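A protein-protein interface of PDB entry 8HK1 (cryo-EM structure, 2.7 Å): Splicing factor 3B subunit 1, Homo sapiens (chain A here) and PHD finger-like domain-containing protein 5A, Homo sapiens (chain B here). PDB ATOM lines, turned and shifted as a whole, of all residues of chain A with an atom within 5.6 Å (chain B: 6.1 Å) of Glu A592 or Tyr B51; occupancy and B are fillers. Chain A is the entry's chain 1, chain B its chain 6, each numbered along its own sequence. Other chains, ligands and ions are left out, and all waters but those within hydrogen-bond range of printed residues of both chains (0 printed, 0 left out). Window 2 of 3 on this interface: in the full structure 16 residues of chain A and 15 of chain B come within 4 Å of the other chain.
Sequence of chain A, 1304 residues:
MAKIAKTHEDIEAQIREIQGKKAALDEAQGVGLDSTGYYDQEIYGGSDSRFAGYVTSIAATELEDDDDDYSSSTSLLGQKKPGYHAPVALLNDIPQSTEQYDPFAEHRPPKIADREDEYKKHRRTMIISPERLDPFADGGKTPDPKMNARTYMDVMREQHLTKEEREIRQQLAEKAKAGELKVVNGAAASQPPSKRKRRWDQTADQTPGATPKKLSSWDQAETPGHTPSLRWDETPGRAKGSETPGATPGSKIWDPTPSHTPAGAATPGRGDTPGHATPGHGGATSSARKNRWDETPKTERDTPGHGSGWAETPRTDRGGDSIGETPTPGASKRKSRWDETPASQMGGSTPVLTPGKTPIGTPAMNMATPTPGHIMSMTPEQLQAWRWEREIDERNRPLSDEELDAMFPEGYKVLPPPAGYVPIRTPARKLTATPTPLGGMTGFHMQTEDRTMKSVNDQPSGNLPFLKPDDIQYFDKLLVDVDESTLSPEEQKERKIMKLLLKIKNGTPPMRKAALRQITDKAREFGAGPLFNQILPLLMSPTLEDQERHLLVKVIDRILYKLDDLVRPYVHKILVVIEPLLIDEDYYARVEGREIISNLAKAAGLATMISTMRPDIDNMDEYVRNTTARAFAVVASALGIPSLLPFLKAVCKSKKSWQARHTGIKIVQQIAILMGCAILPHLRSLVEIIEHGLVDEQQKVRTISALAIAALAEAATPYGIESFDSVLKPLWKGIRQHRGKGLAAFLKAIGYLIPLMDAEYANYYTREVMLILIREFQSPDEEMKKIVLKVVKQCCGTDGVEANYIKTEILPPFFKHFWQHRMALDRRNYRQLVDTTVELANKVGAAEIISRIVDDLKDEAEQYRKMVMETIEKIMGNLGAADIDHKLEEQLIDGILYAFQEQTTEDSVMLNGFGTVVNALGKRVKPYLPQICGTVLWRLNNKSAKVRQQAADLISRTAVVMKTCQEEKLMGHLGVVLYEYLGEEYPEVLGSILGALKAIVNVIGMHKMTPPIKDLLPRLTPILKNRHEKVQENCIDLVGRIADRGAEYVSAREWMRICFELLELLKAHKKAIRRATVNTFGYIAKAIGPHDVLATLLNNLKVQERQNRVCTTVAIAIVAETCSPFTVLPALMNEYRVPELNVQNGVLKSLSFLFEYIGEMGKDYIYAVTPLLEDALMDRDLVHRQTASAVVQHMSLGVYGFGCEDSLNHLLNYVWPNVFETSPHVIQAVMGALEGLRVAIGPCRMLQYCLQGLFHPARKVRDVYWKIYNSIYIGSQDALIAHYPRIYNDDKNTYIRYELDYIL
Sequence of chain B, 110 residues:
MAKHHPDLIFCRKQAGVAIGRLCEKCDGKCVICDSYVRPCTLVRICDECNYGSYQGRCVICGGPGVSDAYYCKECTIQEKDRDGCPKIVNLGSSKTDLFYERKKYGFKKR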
ATOM      1  N   ASP A 546       6.947  27.614   7.448  1.00  0.00           N
ATOM      2  CA  ASP A 546       8.339  27.983   7.686  1.00  0.00           C
ATOM      3  C   ASP A 546       8.535  28.511   9.101  1.00  0.00           C
ATOM      4  O   ASP A 546       9.420  28.045   9.830  1.00  0.00           O
ATOM      5  CB  ASP A 546       8.790  29.019   6.657  1.00  0.00           C
ATOM      6  CG  ASP A 546       8.303  28.700   5.255  1.00  0.00           C
ATOM      7  OD1 ASP A 546       9.150  28.538   4.350  1.00  0.00           O
ATOM      8  OD2 ASP A 546       7.073  28.620   5.056  1.00  0.00           O
ATOM      9  N   ARG A 549       7.897  25.815  11.548  1.00  0.00           N
ATOM     10  CA  ARG A 549       9.099  24.948  11.666  1.00  0.00           C
ATOM     11  C   ARG A 549      10.142  25.666  12.525  1.00  0.00           C
ATOM     12  O   ARG A 549      10.743  25.009  13.386  1.00  0.00           O
ATOM     13  CB  ARG A 549       9.652  24.605  10.280  1.00  0.00           C
ATOM     14  CG  ARG A 549      10.729  23.531  10.297  1.00  0.00           C
ATOM     15  CD  ARG A 549      11.120  23.078   8.903  1.00  0.00           C
ATOM     16  NE  ARG A 549      11.510  24.194   8.056  1.00  0.00           N
ATOM     17  CZ  ARG A 549      11.729  24.100   6.749  1.00  0.00           C
ATOM     18  NH1 ARG A 549      11.592  22.936   6.139  1.00  0.00           N
ATOM     19  NH2 ARG A 549      12.078  25.170   6.058  1.00  0.00           N
ATOM     20  N   HIS A 550      10.302  26.978  12.324  1.00  0.00           N
ATOM     21  CA  HIS A 550      11.292  27.777  13.093  1.00  0.00           C
ATOM     22  C   HIS A 550      10.924  27.761  14.580  1.00  0.00           C
ATOM     23  O   HIS A 550      11.840  27.647  15.412  1.00  0.00           O
ATOM     24  CB  HIS A 550      11.378  29.199  12.525  1.00  0.00           C
ATOM     25  CG  HIS A 550      12.468  30.024  13.116  1.00  0.00           C
ATOM     26  ND1 HIS A 550      13.799  29.825  12.804  1.00  0.00           N
ATOM     27  CD2 HIS A 550      12.435  31.056  13.986  1.00  0.00           C
ATOM     28  CE1 HIS A 550      14.538  30.691  13.463  1.00  0.00           C
ATOM     29  NE2 HIS A 550      13.727  31.460  14.195  1.00  0.00           N
ATOM     30  N   VAL A 553      11.816  24.601  16.195  1.00  0.00           N
ATOM     31  CA  VAL A 553      13.284  24.543  16.462  1.00  0.00           C
ATOM     32  C   VAL A 553      13.567  25.249  17.794  1.00  0.00           C
ATOM     33  O   VAL A 553      14.345  24.699  18.603  1.00  0.00           O
ATOM     34  CB  VAL A 553      14.088  25.171  15.310  1.00  0.00           C
ATOM     35  CG1 VAL A 553      15.573  25.221  15.626  1.00  0.00           C
ATOM     36  CG2 VAL A 553      13.846  24.443  13.998  1.00  0.00           C
ATOM     37  N   TYR A 587      17.356  26.440   1.966  1.00  0.00           N
ATOM     38  CA  TYR A 587      18.478  26.875   2.792  1.00  0.00           C
ATOM     39  C   TYR A 587      18.099  26.931   4.268  1.00  0.00           C
ATOM     40  O   TYR A 587      18.868  26.494   5.135  1.00  0.00           O
ATOM     41  CB  TYR A 587      18.970  28.238   2.305  1.00  0.00           C
ATOM     42  CG  TYR A 587      19.964  28.917   3.214  1.00  0.00           C
ATOM     43  CD1 TYR A 587      21.270  28.461   3.310  1.00  0.00           C
ATOM     44  CD2 TYR A 587      19.597  30.021   3.971  1.00  0.00           C
ATOM     45  CE1 TYR A 587      22.184  29.081   4.138  1.00  0.00           C
ATOM     46  CE2 TYR A 587      20.501  30.647   4.802  1.00  0.00           C
ATOM     47  CZ  TYR A 587      21.792  30.176   4.882  1.00  0.00           C
ATOM     48  OH  TYR A 587      22.697  30.800   5.709  1.00  0.00           O
ATOM     49  N   TYR A 588      16.910  27.450   4.573  1.00  0.00           N
ATOM     50  CA  TYR A 588      16.525  27.638   5.966  1.00  0.00           C
ATOM     51  C   TYR A 588      16.194  26.313   6.635  1.00  0.00           C
ATOM     52  O   TYR A 588      16.403  26.153   7.842  1.00  0.00           O
ATOM     53  CB  TYR A 588      15.347  28.605   6.054  1.00  0.00           C
ATOM     54  CG  TYR A 588      15.695  30.001   5.600  1.00  0.00           C
ATOM     55  CD1 TYR A 588      16.468  30.837   6.391  1.00  0.00           C
ATOM     56  CD2 TYR A 588      15.261  30.481   4.371  1.00  0.00           C
ATOM     57  CE1 TYR A 588      16.792  32.114   5.980  1.00  0.00           C
ATOM     58  CE2 TYR A 588      15.579  31.757   3.948  1.00  0.00           C
ATOM     59  CZ  TYR A 588      16.344  32.569   4.758  1.00  0.00           C
ATOM     60  OH  TYR A 588      16.663  33.839   4.339  1.00  0.00           O
ATOM     61  N   ALA A 589      15.680  25.351   5.865  1.00  0.00           N
ATOM     62  CA  ALA A 589      15.540  23.995   6.381  1.00  0.00           C
ATOM     63  C   ALA A 589      16.889  23.433   6.811  1.00  0.00           C
ATOM     64  O   ALA A 589      16.998  22.792   7.865  1.00  0.00           O
ATOM     65  CB  ALA A 589      14.896  23.103   5.321  1.00  0.00           C
ATOM     66  N   ARG A 590      17.932  23.682   6.018  1.00  0.00           N
ATOM     67  CA  ARG A 590      19.270  23.214   6.367  1.00  0.00           C
ATOM     68  C   ARG A 590      19.782  23.910   7.621  1.00  0.00           C
ATOM     69  O   ARG A 590      20.370  23.271   8.502  1.00  0.00           O
ATOM     70  CB  ARG A 590      20.222  23.443   5.192  1.00  0.00           C
ATOM     71  CG  ARG A 590      19.926  22.583   3.976  1.00  0.00           C
ATOM     72  CD  ARG A 590      21.106  22.557   3.021  1.00  0.00           C
ATOM     73  NE  ARG A 590      21.365  23.872   2.445  1.00  0.00           N
ATOM     74  CZ  ARG A 590      20.988  24.242   1.228  1.00  0.00           C
ATOM     75  NH1 ARG A 590      21.266  25.460   0.783  1.00  0.00           N
ATOM     76  NH2 ARG A 590      20.330  23.394   0.450  1.00  0.00           N
ATOM     77  N   VAL A 591      19.571  25.225   7.716  1.00  0.00           N
ATOM     78  CA  VAL A 591      19.992  25.952   8.913  1.00  0.00           C
ATOM     79  C   VAL A 591      19.289  25.405  10.150  1.00  0.00           C
ATOM     80  O   VAL A 591      19.915  25.204  11.199  1.00  0.00           O
ATOM     81  CB  VAL A 591      19.742  27.463   8.746  1.00  0.00           C
ATOM     82  CG1 VAL A 591      20.288  28.219   9.944  1.00  0.00           C
ATOM     83  CG2 VAL A 591      20.387  27.969   7.471  1.00  0.00           C
ATOM     84  N   GLU A 592      17.983  25.144  10.047  1.00  0.00           N
ATOM     85  CA  GLU A 592      17.233  24.642  11.195  1.00  0.00           C
ATOM     86  C   GLU A 592      17.691  23.243  11.589  1.00  0.00           C
ATOM     87  O   GLU A 592      17.841  22.948  12.780  1.00  0.00           O
ATOM     88  CB  GLU A 592      15.737  24.656  10.884  1.00  0.00           C
ATOM     89  CG  GLU A 592      15.047  25.964  11.237  1.00  0.00           C
ATOM     90  CD  GLU A 592      14.097  26.435  10.153  1.00  0.00           C
ATOM     91  OE1 GLU A 592      13.258  25.627   9.703  1.00  0.00           O
ATOM     92  OE2 GLU A 592      14.188  27.613   9.753  1.00  0.00           O
ATOM     93  N   GLY A 593      17.921  22.370  10.603  1.00  0.00           N
ATOM     94  CA  GLY A 593      18.424  21.044  10.914  1.00  0.00           C
ATOM     95  C   GLY A 593      19.786  21.079  11.578  1.00  0.00           C
ATOM     96  O   GLY A 593      20.048  20.334  12.529  1.00  0.00           O
ATOM     97  N   ARG A 594      20.672  21.956  11.098  1.00  0.00           N
ATOM     98  CA  ARG A 594      21.999  22.057  11.690  1.00  0.00           C
ATOM     99  C   ARG A 594      21.929  22.611  13.107  1.00  0.00           C
ATOM    100  O   ARG A 594      22.659  22.157  13.994  1.00  0.00           O
ATOM    101  CB  ARG A 594      22.901  22.919  10.808  1.00  0.00           C
ATOM    102  CG  ARG A 594      23.321  22.223   9.525  1.00  0.00           C
ATOM    103  CD  ARG A 594      24.514  22.895   8.880  1.00  0.00           C
ATOM    104  NE  ARG A 594      24.291  23.134   7.458  1.00  0.00           N
ATOM    105  CZ  ARG A 594      23.929  24.307   6.945  1.00  0.00           C
ATOM    106  NH1 ARG A 594      23.751  25.355   7.735  1.00  0.00           N
ATOM    107  NH2 ARG A 594      23.747  24.428   5.638  1.00  0.00           N
ATOM    108  N   GLU A 595      21.039  23.578  13.348  1.00  0.00           N
ATOM    109  CA  GLU A 595      20.864  24.093  14.703  1.00  0.00           C
ATOM    110  C   GLU A 595      20.334  23.016  15.641  1.00  0.00           C
ATOM    111  O   GLU A 595      20.797  22.891  16.783  1.00  0.00           O
ATOM    112  CB  GLU A 595      19.927  25.299  14.686  1.00  0.00           C
ATOM    113  CG  GLU A 595      19.629  25.866  16.061  1.00  0.00           C
ATOM    114  CD  GLU A 595      18.756  27.102  16.005  1.00  0.00           C
ATOM    115  OE1 GLU A 595      17.928  27.205  15.076  1.00  0.00           O
ATOM    116  OE2 GLU A 595      18.893  27.972  16.893  1.00  0.00           O
ATOM    117  N   ILE A 596      19.371  22.220  15.171  1.00  0.00           N
ATOM    118  CA  ILE A 596      18.823  21.144  15.994  1.00  0.00           C
ATOM    119  C   ILE A 596      19.908  20.134  16.337  1.00  0.00           C
ATOM    120  O   ILE A 596      20.052  19.718  17.492  1.00  0.00           O
ATOM    121  CB  ILE A 596      17.630  20.479  15.288  1.00  0.00           C
ATOM    122  CG1 ILE A 596      16.421  21.415  15.278  1.00  0.00           C
ATOM    123  CG2 ILE A 596      17.276  19.161  15.962  1.00  0.00           C
ATOM    124  CD1 ILE A 596      15.157  20.774  14.751  1.00  0.00           C
ATOM    125  N   ILE A 597      20.691  19.720  15.336  1.00  0.00           N
ATOM    126  CA  ILE A 597      21.738  18.731  15.586  1.00  0.00           C
ATOM    127  C   ILE A 597      22.814  19.304  16.502  1.00  0.00           C
ATOM    128  O   ILE A 597      23.379  18.592  17.336  1.00  0.00           O
ATOM    129  CB  ILE A 597      22.323  18.224  14.257  1.00  0.00           C
ATOM    130  CG1 ILE A 597      21.263  17.442  13.480  1.00  0.00           C
ATOM    131  CG2 ILE A 597      23.540  17.346  14.500  1.00  0.00           C
ATOM    132  CD1 ILE A 597      21.800  16.728  12.269  1.00  0.00           C
ATOM    133  N   ASP B  47      17.391  40.466  13.931  1.00  0.00           N
ATOM    134  CA  ASP B  47      17.517  39.195  13.231  1.00  0.00           C
ATOM    135  C   ASP B  47      16.224  38.396  13.163  1.00  0.00           C
ATOM    136  O   ASP B  47      16.073  37.586  12.244  1.00  0.00           O
ATOM    137  CB  ASP B  47      18.601  38.331  13.889  1.00  0.00           C
ATOM    138  CG  ASP B  47      20.003  38.815  13.580  1.00  0.00           C
ATOM    139  OD1 ASP B  47      20.205  39.427  12.513  1.00  0.00           O
ATOM    140  OD2 ASP B  47      20.907  38.573  14.407  1.00  0.00           O
ATOM    141  N   GLU B  48      15.292  38.587  14.098  1.00  0.00           N
ATOM    142  CA  GLU B  48      14.032  37.858  14.015  1.00  0.00           C
ATOM    143  C   GLU B  48      13.092  38.499  13.004  1.00  0.00           C
ATOM    144  O   GLU B  48      12.190  37.833  12.483  1.00  0.00           O
ATOM    145  CB  GLU B  48      13.375  37.755  15.395  1.00  0.00           C
ATOM    146  CG  GLU B  48      12.807  39.052  15.954  1.00  0.00           C
ATOM    147  CD  GLU B  48      11.311  39.197  15.714  1.00  0.00           C
ATOM    148  OE1 GLU B  48      10.883  40.272  15.248  1.00  0.00           O
ATOM    149  OE2 GLU B  48      10.563  38.239  15.997  1.00  0.00           O
ATOM    150  N   CYS B  49      13.284  39.786  12.713  1.00  0.00           N
ATOM    151  CA  CYS B  49      12.539  40.442  11.646  1.00  0.00           C
ATOM    152  C   CYS B  49      13.098  40.126  10.266  1.00  0.00           C
ATOM    153  O   CYS B  49      12.402  40.331   9.267  1.00  0.00           O
ATOM    154  CB  CYS B  49      12.532  41.959  11.857  1.00  0.00           C
ATOM    155  SG  CYS B  49      11.494  42.537  13.220  1.00  0.00           S
ATOM    156  N   ASN B  50      14.337  39.647  10.189  1.00  0.00           N
ATOM    157  CA  ASN B  50      14.987  39.310   8.925  1.00  0.00           C
ATOM    158  C   ASN B  50      15.330  37.825   8.976  1.00  0.00           C
ATOM    159  O   ASN B  50      16.448  37.442   9.323  1.00  0.00           O
ATOM    160  CB  ASN B  50      16.232  40.169   8.728  1.00  0.00           C
ATOM    161  CG  ASN B  50      16.713  40.191   7.295  1.00  0.00           C
ATOM    162  OD1 ASN B  50      16.033  40.706   6.413  1.00  0.00           O
ATOM    163  ND2 ASN B  50      17.894  39.638   7.056  1.00  0.00           N
ATOM    164  N   TYR B  51      14.368  36.979   8.618  1.00  0.00           N
ATOM    165  CA  TYR B  51      14.598  35.543   8.681  1.00  0.00           C
ATOM    166  C   TYR B  51      13.563  34.816   7.838  1.00  0.00           C
ATOM    167  O   TYR B  51      12.365  35.077   7.956  1.00  0.00           O
ATOM    168  CB  TYR B  51      14.551  35.033  10.126  1.00  0.00           C
ATOM    169  CG  TYR B  51      14.782  33.546  10.249  1.00  0.00           C
ATOM    170  CD1 TYR B  51      16.066  33.030  10.336  1.00  0.00           C
ATOM    171  CD2 TYR B  51      13.716  32.659  10.268  1.00  0.00           C
ATOM    172  CE1 TYR B  51      16.283  31.669  10.441  1.00  0.00           C
ATOM    173  CE2 TYR B  51      13.921  31.299  10.371  1.00  0.00           C
ATOM    174  CZ  TYR B  51      15.205  30.809  10.458  1.00  0.00           C
ATOM    175  OH  TYR B  51      15.413  29.452  10.565  1.00  0.00           O
ATOM    176  N   GLY B  52      14.039  33.894   7.006  1.00  0.00           N
ATOM    177  CA  GLY B  52      13.148  33.016   6.266  1.00  0.00           C
ATOM    178  C   GLY B  52      12.223  33.789   5.348  1.00  0.00           C
ATOM    179  O   GLY B  52      12.658  34.481   4.421  1.00  0.00           O
ATOM    180  N   SER B  53      10.918  33.674   5.608  1.00  0.00           N
ATOM    181  CA  SER B  53       9.934  34.365   4.785  1.00  0.00           C
ATOM    182  C   SER B  53       9.925  35.862   5.056  1.00  0.00           C
ATOM    183  O   SER B  53       9.413  36.637   4.240  1.00  0.00           O
ATOM    184  CB  SER B  53       8.544  33.776   5.028  1.00  0.00           C
ATOM    185  OG  SER B  53       8.615  32.383   5.258  1.00  0.00           O
ATOM    186  N   TYR B  54      10.478  36.287   6.188  1.00  0.00           N
ATOM    187  CA  TYR B  54      10.519  37.692   6.561  1.00  0.00           C
ATOM    188  C   TYR B  54      11.725  38.424   5.990  1.00  0.00           C
ATOM    189  O   TYR B  54      11.983  39.563   6.387  1.00  0.00           O
ATOM    190  CB  TYR B  54      10.521  37.837   8.087  1.00  0.00           C
ATOM    191  CG  TYR B  54       9.407  37.107   8.807  1.00  0.00           C
ATOM    192  CD1 TYR B  54       8.183  36.875   8.196  1.00  0.00           C
ATOM    193  CD2 TYR B  54       9.581  36.663  10.112  1.00  0.00           C
ATOM    194  CE1 TYR B  54       7.168  36.213   8.858  1.00  0.00           C
ATOM    195  CE2 TYR B  54       8.574  36.005  10.782  1.00  0.00           C
ATOM    196  CZ  TYR B  54       7.370  35.782  10.151  1.00  0.00           C
ATOM    197  OH  TYR B  54       6.363  35.121  10.817  1.00  0.00           O
ATOM    198  N   GLN B  55      12.466  37.801   5.068  1.00  0.00           N
ATOM    199  CA  GLN B  55      13.757  38.345   4.658  1.00  0.00           C
ATOM    200  C   GLN B  55      13.611  39.714   4.002  1.00  0.00           C
ATOM    201  O   GLN B  55      14.272  40.679   4.399  1.00  0.00           O
ATOM    202  CB  GLN B  55      14.460  37.372   3.714  1.00  0.00           C
ATOM    203  CG  GLN B  55      15.963  37.559   3.674  1.00  0.00           C
ATOM    204  CD  GLN B  55      16.405  38.489   2.566  1.00  0.00           C
ATOM    205  OE1 GLN B  55      15.821  38.511   1.484  1.00  0.00           O
ATOM    206  NE2 GLN B  55      17.446  39.270   2.833  1.00  0.00           N
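A ring nitrogen (ND1) of His A550 is in hydrogen-bond range of the side-chain hydroxyl (OH) of Tyr B51 (2.8 Å).
OE2 of Glu A592 lies close to OH of Tyr B51 (2.4 Å).
NE of Arg A549 lies within salt-bridge range of OE1 of Glu A592 (2.8 Å).
The side-chain amide oxygen (OD1) of Asn B50 lies close to the backbone carbonyl oxygen (O) of Gln B55 (2.7 Å).
CB of Asp A546 touches OG of Ser B53, 3.6 Å away.
CE1 of Tyr A588 touches N of Gly B52 (3.4 Å).
Tyr A588 touches Gln B55 (OH to CG, 3.8 Å).
Printed residues of chain A within 4 Å of Tyr B51: His A550 (2.8 Å) and Glu A592 (2.4 Å).
Of the printed residues of chain B, Tyr A588 touches Gly B52 (3.4 Å) and Gln B55 (3.8 Å).
Printed residues of chain A within 4 Å of Gln B55: Tyr A588.
Of the printed residues of chain B, His A550 touches Tyr B51 (2.8 Å).
Printed residues of chain B within 4 Å of Asp A546: Ser B53 (3.6 Å).
Of the printed residues of chain A, Gly B52 touches Tyr A588 (3.4 Å).
Val A553 touches none of the printed residues of chain B.
The nearest printed residue of chain B that does not touch Asp A546 is Tyr B51 (5.6 Å).
Printed residues of chain B that touch a printed residue of chain A: Tyr B51, Gly B52, Ser B53 and Gln B55.
Hydrophobic or aromatic side chains of chain A that line the printed part of chain B: His A550 and Tyr A588.
Among the printed residues, 5 pairs touch across the chains.
Among the printed residues, no Asp or Glu carboxylate lies within 4 Å of a Lys or Arg side-chain nitrogen of the other chain.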
